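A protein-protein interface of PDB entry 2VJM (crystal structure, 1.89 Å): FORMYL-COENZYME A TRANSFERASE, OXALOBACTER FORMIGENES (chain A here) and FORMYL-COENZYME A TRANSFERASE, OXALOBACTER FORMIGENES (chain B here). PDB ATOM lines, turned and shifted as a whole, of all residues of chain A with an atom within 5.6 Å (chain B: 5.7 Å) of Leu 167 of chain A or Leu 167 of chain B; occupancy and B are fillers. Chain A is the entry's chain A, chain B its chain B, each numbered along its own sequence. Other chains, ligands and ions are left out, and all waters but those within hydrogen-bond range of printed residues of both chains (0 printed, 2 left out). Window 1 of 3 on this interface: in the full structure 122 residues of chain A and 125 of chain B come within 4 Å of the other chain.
O of Leu 207 of chain B sits at hydrogen-bond distance from N of Ala 166 of chain A (2.8 Å). The backbone carbonyl oxygen (O) of Leu 207 of chain A lies within hydrogen-bond range of the backbone NH (N) of Ala 166 of chain B, 2.9 Å away.
N of Leu 167 of chain A is in hydrogen-bond range of OE1 of Glu 140 of chain A, at 3.3 Å. O of Leu 167 of chain A sits at hydrogen-bond distance from ND2 of Asn 171 of chain A, 3.0 Å away. N of Leu 167 of chain B sits at hydrogen-bond distance from OE2 of Glu 140 of chain B, 3.2 Å away. OE1 of Gln 144 of chain B sits at hydrogen-bond distance from N of Ser 163 of chain B (2.8 Å). O of Ala 165 of chain B lies within hydrogen-bond range of NE2 of Gln 144 of chain B (3.2 Å). ND2 of Asn 171 of chain B is in hydrogen-bond range of O of Leu 167 of chain B (2.9 Å).
Among the printed residues, pairs that only touch across the chains: Leu 167 of chain A with Leu 167 of chain B (3.2 Å), Leu 207 of chain A with Asn 171 of chain B (3.6 Å), Leu 167 of chain A with Ala 165 of chain B (3.6 Å), Asn 171 of chain A with Leu 207 of chain B (3.6 Å), Ala 165 of chain A with Leu 207 of chain B (3.6 Å), Ala 165 of chain A with Leu 167 of chain B (3.7 Å), Leu 207 of chain A with Ala 165 of chain B (3.7 Å), Leu 167 of chain A with Ser 163 of chain B (3.8 Å), Ser 163 of chain A with Ser 163 of chain B (3.9 Å) and Ser 170 of chain A with Leu 207 of chain B (3.96 Å).
Of chain B, only Ser 163 (3.8 Å), Ala 165 (3.6 Å) and Leu 167 (3.2 Å) come within 4 Å of Leu 167 of chain A. Of chain A, only Ala 165 (3.7 Å) and Leu 167 (3.2 Å) come within 4 Å of Leu 167 of chain B. Of the printed residues of chain B, Asn 171 of chain A touches Leu 207. Printed residues of chain A within 4 Å of Asn 171 of chain B: Leu 207 (3.6 Å). Of the printed residues of chain A, Ala 165 of chain B touches Leu 167 and Leu 207. Of the printed residues of chain B, Leu 207 of chain A touches Ala 165 (3.7 Å), Ala 166 (2.9 Å) and Asn 171 (3.6 Å). Printed residues of chain B within 4 Å of Ser 170 of chain A: Leu 207. The nearest residue of chain B that does not touch Leu 167 of chain A is Leu 207 of chain B (4.6 Å). The nearest printed residue of chain B that does not touch Ser 170 of chain A is Asn 171 of chain B (7.3 Å).
Of the 16 printed residues of chain A, 7 touch a printed residue of chain B. Hydrophobic or aromatic side chains of chain A within 4 Å of the printed part of chain B: Ala 165, Ala 166, Leu 167 and Leu 207. Among the printed residues, 12 pairs touch across the chains.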
ATOM      1  N   GLU A 140      -4.965 -16.297 -12.214  1.00  0.00           N
ATOM      2  CA  GLU A 140      -5.631 -17.584 -11.941  1.00  0.00           C
ATOM      3  C   GLU A 140      -5.478 -18.108 -10.506  1.00  0.00           C
ATOM      4  O   GLU A 140      -6.464 -18.209  -9.768  1.00  0.00           O
ATOM      5  CB  GLU A 140      -5.116 -18.656 -12.922  1.00  0.00           C
ATOM      6  CG  GLU A 140      -5.568 -20.096 -12.621  1.00  0.00           C
ATOM      7  CD  GLU A 140      -7.068 -20.259 -12.708  1.00  0.00           C
ATOM      8  OE1 GLU A 140      -7.664 -20.839 -11.778  1.00  0.00           O
ATOM      9  OE2 GLU A 140      -7.660 -19.791 -13.705  1.00  0.00           O
ATOM     10  N   GLN A 144      -7.950 -18.507  -7.072  1.00  0.00           N
ATOM     11  CA  GLN A 144      -8.237 -19.780  -6.384  1.00  0.00           C
ATOM     12  C   GLN A 144      -7.969 -19.655  -4.878  1.00  0.00           C
ATOM     13  O   GLN A 144      -8.727 -20.174  -4.049  1.00  0.00           O
ATOM     14  CB  GLN A 144      -7.401 -20.928  -6.965  1.00  0.00           C
ATOM     15  CG  GLN A 144      -7.800 -21.367  -8.380  1.00  0.00           C
ATOM     16  CD  GLN A 144      -7.230 -22.726  -8.756  1.00  0.00           C
ATOM     17  OE1 GLN A 144      -7.006 -23.577  -7.892  1.00  0.00           O
ATOM     18  NE2 GLN A 144      -7.000 -22.940 -10.048  1.00  0.00           N
ATOM     19  N   ALA A 149     -10.782 -22.173  -2.518  1.00  0.00           N
ATOM     20  CA  ALA A 149     -10.438 -23.444  -3.183  1.00  0.00           C
ATOM     21  C   ALA A 149      -9.072 -24.000  -2.756  1.00  0.00           C
ATOM     22  O   ALA A 149      -8.956 -25.180  -2.434  1.00  0.00           O
ATOM     23  CB  ALA A 149     -10.487 -23.280  -4.708  1.00  0.00           C
ATOM     24  N   SER A 163      -5.916 -26.057  -8.128  1.00  0.00           N
ATOM     25  CA  SER A 163      -6.585 -27.010  -9.010  1.00  0.00           C
ATOM     26  C   SER A 163      -6.075 -26.854 -10.434  1.00  0.00           C
ATOM     27  O   SER A 163      -5.785 -25.739 -10.875  1.00  0.00           O
ATOM     28  CB  SER A 163      -8.098 -26.781  -8.996  1.00  0.00           C
ATOM     29  OG  SER A 163      -8.726 -27.448 -10.078  1.00  0.00           O
ATOM     30  N   ALA A 165      -7.931 -27.402 -12.949  1.00  0.00           N
ATOM     31  CA  ALA A 165      -9.048 -26.724 -13.606  1.00  0.00           C
ATOM     32  C   ALA A 165      -8.947 -25.217 -13.391  1.00  0.00           C
ATOM     33  O   ALA A 165      -8.559 -24.769 -12.311  1.00  0.00           O
ATOM     34  CB  ALA A 165     -10.379 -27.244 -13.070  1.00  0.00           C
ATOM     35  N   ALA A 166      -9.315 -24.453 -14.420  1.00  0.00           N
ATOM     36  CA  ALA A 166      -9.257 -22.993 -14.396  1.00  0.00           C
ATOM     37  C   ALA A 166     -10.409 -22.381 -13.586  1.00  0.00           C
ATOM     38  O   ALA A 166     -11.308 -21.737 -14.144  1.00  0.00           O
ATOM     39  CB  ALA A 166      -9.265 -22.459 -15.827  1.00  0.00           C
ATOM     40  N   LEU A 167     -10.362 -22.593 -12.273  1.00  0.00           N
ATOM     41  CA  LEU A 167     -11.366 -22.103 -11.321  1.00  0.00           C
ATOM     42  C   LEU A 167     -11.414 -20.575 -11.263  1.00  0.00           C
ATOM     43  O   LEU A 167     -12.458 -19.987 -11.006  1.00  0.00           O
ATOM     44  CB  LEU A 167     -11.054 -22.624  -9.910  1.00  0.00           C
ATOM     45  CG  LEU A 167     -11.225 -24.099  -9.564  1.00  0.00           C
ATOM     46  CD1 LEU A 167     -10.874 -24.316  -8.081  1.00  0.00           C
ATOM     47  CD2 LEU A 167     -12.655 -24.553  -9.849  1.00  0.00           C
ATOM     48  N   GLY A 168     -10.260 -19.946 -11.460  1.00  0.00           N
ATOM     49  CA  GLY A 168     -10.165 -18.495 -11.466  1.00  0.00           C
ATOM     50  C   GLY A 168     -10.611 -17.874 -12.777  1.00  0.00           C
ATOM     51  O   GLY A 168     -11.422 -16.958 -12.782  1.00  0.00           O
ATOM     52  N   ASP A 169     -10.084 -18.380 -13.892  1.00  0.00           N
ATOM     53  CA  ASP A 169     -10.239 -17.703 -15.184  1.00  0.00           C
ATOM     54  C   ASP A 169     -11.421 -18.208 -15.996  1.00  0.00           C
ATOM     55  O   ASP A 169     -12.431 -17.516 -16.084  1.00  0.00           O
ATOM     56  CB  ASP A 169      -8.944 -17.815 -15.982  1.00  0.00           C
ATOM     57  CG  ASP A 169      -7.995 -16.736 -15.511  1.00  0.00           C
ATOM     58  OD1 ASP A 169      -7.304 -16.925 -14.530  1.00  0.00           O
ATOM     59  N   SER A 170     -11.310 -19.388 -16.607  1.00  0.00           N
ATOM     60  CA  SER A 170     -12.394 -19.905 -17.446  1.00  0.00           C
ATOM     61  C   SER A 170     -13.715 -19.951 -16.687  1.00  0.00           C
ATOM     62  O   SER A 170     -14.757 -19.585 -17.228  1.00  0.00           O
ATOM     63  CB  SER A 170     -12.071 -21.291 -18.017  1.00  0.00           C
ATOM     64  OG  SER A 170     -11.217 -21.195 -19.141  1.00  0.00           O
ATOM     65  N   ASN A 171     -13.665 -20.397 -15.431  1.00  0.00           N
ATOM     66  CA  ASN A 171     -14.856 -20.421 -14.568  1.00  0.00           C
ATOM     67  C   ASN A 171     -15.516 -19.041 -14.441  1.00  0.00           C
ATOM     68  O   ASN A 171     -16.740 -18.913 -14.528  1.00  0.00           O
ATOM     69  CB  ASN A 171     -14.479 -20.964 -13.183  1.00  0.00           C
ATOM     70  CG  ASN A 171     -15.638 -20.949 -12.199  1.00  0.00           C
ATOM     71  OD1 ASN A 171     -16.765 -21.283 -12.551  1.00  0.00           O
ATOM     72  ND2 ASN A 171     -15.353 -20.573 -10.950  1.00  0.00           N
ATOM     73  N   SER A 172     -14.706 -18.004 -14.263  1.00  0.00           N
ATOM     74  CA  SER A 172     -15.235 -16.643 -14.185  1.00  0.00           C
ATOM     75  C   SER A 172     -15.866 -16.205 -15.514  1.00  0.00           C
ATOM     76  O   SER A 172     -16.915 -15.567 -15.523  1.00  0.00           O
ATOM     77  CB  SER A 172     -14.150 -15.663 -13.752  1.00  0.00           C
ATOM     78  OG  SER A 172     -13.696 -15.975 -12.444  1.00  0.00           O
ATOM     79  N   MET A 200     -13.628 -12.761  -9.931  1.00  0.00           N
ATOM     80  CA  MET A 200     -12.989 -14.074  -9.906  1.00  0.00           C
ATOM     81  C   MET A 200     -13.118 -14.739  -8.531  1.00  0.00           C
ATOM     82  O   MET A 200     -13.372 -15.946  -8.439  1.00  0.00           O
ATOM     83  CB  MET A 200     -11.517 -13.948 -10.314  1.00  0.00           C
ATOM     84  CG  MET A 200     -11.324 -13.493 -11.767  1.00  0.00           C
ATOM     85  SD  MET A 200      -9.642 -12.918 -12.079  1.00  0.00           S
ATOM     86  CE  MET A 200      -8.835 -14.491 -12.326  1.00  0.00           C
ATOM     87  N   ALA A 203     -16.780 -16.086  -8.376  1.00  0.00           N
ATOM     88  CA  ALA A 203     -16.934 -17.282  -9.203  1.00  0.00           C
ATOM     89  C   ALA A 203     -16.312 -18.523  -8.534  1.00  0.00           C
ATOM     90  O   ALA A 203     -16.895 -19.610  -8.586  1.00  0.00           O
ATOM     91  CB  ALA A 203     -16.338 -17.053 -10.604  1.00  0.00           C
ATOM     92  N   VAL A 204     -15.147 -18.356  -7.903  1.00  0.00           N
ATOM     93  CA  VAL A 204     -14.510 -19.435  -7.153  1.00  0.00           C
ATOM     94  C   VAL A 204     -15.366 -19.812  -5.945  1.00  0.00           C
ATOM     95  O   VAL A 204     -15.653 -20.995  -5.732  1.00  0.00           O
ATOM     96  CB  VAL A 204     -13.073 -19.074  -6.693  1.00  0.00           C
ATOM     97  CG1 VAL A 204     -12.516 -20.152  -5.752  1.00  0.00           C
ATOM     98  CG2 VAL A 204     -12.148 -18.880  -7.910  1.00  0.00           C
ATOM     99  N   LEU A 207     -18.402 -22.018  -6.618  1.00  0.00           N
ATOM    100  CA  LEU A 207     -18.105 -23.452  -6.755  1.00  0.00           C
ATOM    101  C   LEU A 207     -17.699 -24.108  -5.424  1.00  0.00           C
ATOM    102  O   LEU A 207     -17.828 -25.316  -5.263  1.00  0.00           O
ATOM    103  CB  LEU A 207     -17.033 -23.695  -7.826  1.00  0.00           C
ATOM    104  CG  LEU A 207     -17.393 -23.295  -9.263  1.00  0.00           C
ATOM    105  CD1 LEU A 207     -16.330 -23.821 -10.214  1.00  0.00           C
ATOM    106  CD2 LEU A 207     -18.797 -23.798  -9.670  1.00  0.00           C
ATOM    107  N   GLU B 140     -20.058 -36.020  -8.141  1.00  0.00           N
ATOM    108  CA  GLU B 140     -18.951 -35.045  -8.135  1.00  0.00           C
ATOM    109  C   GLU B 140     -17.569 -35.537  -8.589  1.00  0.00           C
ATOM    110  O   GLU B 140     -17.104 -35.207  -9.691  1.00  0.00           O
ATOM    111  CB  GLU B 140     -18.837 -34.447  -6.716  1.00  0.00           C
ATOM    112  CG  GLU B 140     -17.709 -33.411  -6.514  1.00  0.00           C
ATOM    113  CD  GLU B 140     -17.826 -32.224  -7.446  1.00  0.00           C
ATOM    114  OE1 GLU B 140     -18.872 -31.545  -7.407  1.00  0.00           O
ATOM    115  OE2 GLU B 140     -16.867 -31.958  -8.211  1.00  0.00           O
ATOM    116  N   GLN B 144     -14.918 -35.300 -11.882  1.00  0.00           N
ATOM    117  CA  GLN B 144     -13.589 -34.685 -11.819  1.00  0.00           C
ATOM    118  C   GLN B 144     -12.530 -35.619 -12.424  1.00  0.00           C
ATOM    119  O   GLN B 144     -11.614 -35.174 -13.123  1.00  0.00           O
ATOM    120  CB  GLN B 144     -13.208 -34.332 -10.378  1.00  0.00           C
ATOM    121  CG  GLN B 144     -14.062 -33.230  -9.753  1.00  0.00           C
ATOM    122  CD  GLN B 144     -13.340 -32.505  -8.626  1.00  0.00           C
ATOM    123  OE1 GLN B 144     -12.108 -32.516  -8.560  1.00  0.00           O
ATOM    124  NE2 GLN B 144     -14.101 -31.852  -7.751  1.00  0.00           N
ATOM    125  N   ALA B 149      -9.422 -33.345 -14.652  1.00  0.00           N
ATOM    126  CA  ALA B 149      -8.997 -32.505 -13.523  1.00  0.00           C
ATOM    127  C   ALA B 149      -8.144 -33.274 -12.501  1.00  0.00           C
ATOM    128  O   ALA B 149      -7.076 -32.804 -12.091  1.00  0.00           O
ATOM    129  CB  ALA B 149     -10.214 -31.869 -12.847  1.00  0.00           C
ATOM    130  N   SER B 163     -10.473 -31.530  -6.577  1.00  0.00           N
ATOM    131  CA  SER B 163     -10.595 -30.151  -6.122  1.00  0.00           C
ATOM    132  C   SER B 163     -11.670 -30.072  -5.042  1.00  0.00           C
ATOM    133  O   SER B 163     -12.646 -30.820  -5.076  1.00  0.00           O
ATOM    134  CB  SER B 163     -10.962 -29.230  -7.291  1.00  0.00           C
ATOM    135  OG  SER B 163     -11.131 -27.889  -6.854  1.00  0.00           O
ATOM    136  N   ALA B 165     -13.405 -27.401  -4.873  1.00  0.00           N
ATOM    137  CA  ALA B 165     -14.451 -26.789  -5.695  1.00  0.00           C
ATOM    138  C   ALA B 165     -15.288 -27.853  -6.386  1.00  0.00           C
ATOM    139  O   ALA B 165     -14.762 -28.886  -6.834  1.00  0.00           O
ATOM    140  CB  ALA B 165     -13.846 -25.844  -6.737  1.00  0.00           C
ATOM    141  N   ALA B 166     -16.587 -27.582  -6.497  1.00  0.00           N
ATOM    142  CA  ALA B 166     -17.542 -28.519  -7.090  1.00  0.00           C
ATOM    143  C   ALA B 166     -17.473 -28.456  -8.618  1.00  0.00           C
ATOM    144  O   ALA B 166     -18.402 -27.966  -9.275  1.00  0.00           O
ATOM    145  CB  ALA B 166     -18.947 -28.210  -6.606  1.00  0.00           C
ATOM    146  N   LEU B 167     -16.352 -28.932  -9.163  1.00  0.00           N
ATOM    147  CA  LEU B 167     -16.110 -28.979 -10.605  1.00  0.00           C
ATOM    148  C   LEU B 167     -17.106 -29.888 -11.324  1.00  0.00           C
ATOM    149  O   LEU B 167     -17.485 -29.638 -12.465  1.00  0.00           O
ATOM    150  CB  LEU B 167     -14.705 -29.506 -10.897  1.00  0.00           C
ATOM    151  CG  LEU B 167     -13.496 -28.699 -10.457  1.00  0.00           C
ATOM    152  CD1 LEU B 167     -12.221 -29.469 -10.804  1.00  0.00           C
ATOM    153  CD2 LEU B 167     -13.507 -27.338 -11.129  1.00  0.00           C
ATOM    154  N   GLY B 168     -17.510 -30.955 -10.652  1.00  0.00           N
ATOM    155  CA  GLY B 168     -18.494 -31.878 -11.200  1.00  0.00           C
ATOM    156  C   GLY B 168     -19.925 -31.381 -11.053  1.00  0.00           C
ATOM    157  O   GLY B 168     -20.690 -31.428 -12.009  1.00  0.00           O
ATOM    158  N   A0A B 169     -20.290 -30.913  -9.860  1.00  0.00           N
ATOM    159  CA  A0A B 169     -21.704 -30.637  -9.523  1.00  0.00           C
ATOM    160  C   A0A B 169     -22.127 -29.205  -9.846  1.00  0.00           C
ATOM    161  O   A0A B 169     -22.728 -28.956 -10.891  1.00  0.00           O
ATOM    162  CB  A0A B 169     -21.948 -30.949  -8.040  1.00  0.00           C
ATOM    163  CG  A0A B 169     -21.836 -32.411  -7.641  1.00  0.00           C
ATOM    164  OD1 A0A B 169     -21.639 -33.313  -8.454  1.00  0.00           O
ATOM    165  OD2 A0A B 169     -21.936 -32.737  -6.220  1.00  0.00           O
ATOM    166  CM1 A0A B 169     -22.942 -33.733  -5.851  1.00  0.00           C
ATOM    167  OM2 A0A B 169     -22.770 -34.917  -6.115  1.00  0.00           O
ATOM    168  N   SER B 170     -21.831 -28.248  -8.968  1.00  0.00           N
ATOM    169  CA  SER B 170     -22.281 -26.870  -9.191  1.00  0.00           C
ATOM    170  C   SER B 170     -21.815 -26.300 -10.537  1.00  0.00           C
ATOM    171  O   SER B 170     -22.567 -25.594 -11.199  1.00  0.00           O
ATOM    172  CB  SER B 170     -21.837 -25.952  -8.050  1.00  0.00           C
ATOM    173  OG  SER B 170     -22.650 -26.155  -6.907  1.00  0.00           O
ATOM    174  N   ASN B 171     -20.582 -26.615 -10.930  1.00  0.00           N
ATOM    175  CA  ASN B 171     -20.041 -26.196 -12.226  1.00  0.00           C
ATOM    176  C   ASN B 171     -20.915 -26.676 -13.397  1.00  0.00           C
ATOM    177  O   ASN B 171     -21.208 -25.920 -14.331  1.00  0.00           O
ATOM    178  CB  ASN B 171     -18.602 -26.707 -12.365  1.00  0.00           C
ATOM    179  CG  ASN B 171     -18.001 -26.442 -13.731  1.00  0.00           C
ATOM    180  OD1 ASN B 171     -18.089 -25.333 -14.249  1.00  0.00           O
ATOM    181  ND2 ASN B 171     -17.371 -27.469 -14.318  1.00  0.00           N
ATOM    182  N   SER B 172     -21.351 -27.929 -13.333  1.00  0.00           N
ATOM    183  CA  SER B 172     -22.266 -28.458 -14.346  1.00  0.00           C
ATOM    184  C   SER B 172     -23.601 -27.719 -14.321  1.00  0.00           C
ATOM    185  O   SER B 172     -24.160 -27.411 -15.371  1.00  0.00           O
ATOM    186  CB  SER B 172     -22.462 -29.960 -14.172  1.00  0.00           C
ATOM    187  OG  SER B 172     -21.236 -30.623 -14.383  1.00  0.00           O
ATOM    188  N   MET B 200     -21.566 -33.794 -16.995  1.00  0.00           N
ATOM    189  CA  MET B 200     -20.600 -33.427 -15.955  1.00  0.00           C
ATOM    190  C   MET B 200     -19.150 -33.545 -16.440  1.00  0.00           C
ATOM    191  O   MET B 200     -18.326 -32.672 -16.144  1.00  0.00           O
ATOM    192  CB  MET B 200     -20.827 -34.257 -14.685  1.00  0.00           C
ATOM    193  CG  MET B 200     -22.186 -33.984 -14.024  1.00  0.00           C
ATOM    194  SD  MET B 200     -22.711 -35.274 -12.877  1.00  0.00           S
ATOM    195  CE  MET B 200     -21.567 -35.017 -11.539  1.00  0.00           C
ATOM    196  N   ALA B 203     -18.447 -30.419 -18.623  1.00  0.00           N
ATOM    197  CA  ALA B 203     -18.328 -29.194 -17.826  1.00  0.00           C
ATOM    198  C   ALA B 203     -16.951 -29.135 -17.156  1.00  0.00           C
ATOM    199  O   ALA B 203     -16.311 -28.079 -17.123  1.00  0.00           O
ATOM    200  CB  ALA B 203     -19.456 -29.112 -16.783  1.00  0.00           C
ATOM    201  N   VAL B 204     -16.488 -30.280 -16.649  1.00  0.00           N
ATOM    202  CA  VAL B 204     -15.146 -30.381 -16.093  1.00  0.00           C
ATOM    203  C   VAL B 204     -14.088 -30.102 -17.180  1.00  0.00           C
ATOM    204  O   VAL B 204     -13.184 -29.280 -16.975  1.00  0.00           O
ATOM    205  CB  VAL B 204     -14.895 -31.765 -15.426  1.00  0.00           C
ATOM    206  CG1 VAL B 204     -13.429 -31.914 -15.032  1.00  0.00           C
ATOM    207  CG2 VAL B 204     -15.799 -31.948 -14.178  1.00  0.00           C
ATOM    208  N   LEU B 207     -13.398 -26.470 -18.126  1.00  0.00           N
ATOM    209  CA  LEU B 207     -12.487 -25.809 -17.196  1.00  0.00           C
ATOM    210  C   LEU B 207     -11.044 -26.314 -17.277  1.00  0.00           C
ATOM    211  O   LEU B 207     -10.134 -25.614 -16.844  1.00  0.00           O
ATOM    212  CB  LEU B 207     -13.008 -25.899 -15.749  1.00  0.00           C
ATOM    213  CG  LEU B 207     -14.364 -25.225 -15.488  1.00  0.00           C
ATOM    214  CD1 LEU B 207     -14.655 -25.167 -13.971  1.00  0.00           C
ATOM    215  CD2 LEU B 207     -14.443 -23.822 -16.107  1.00  0.00           C
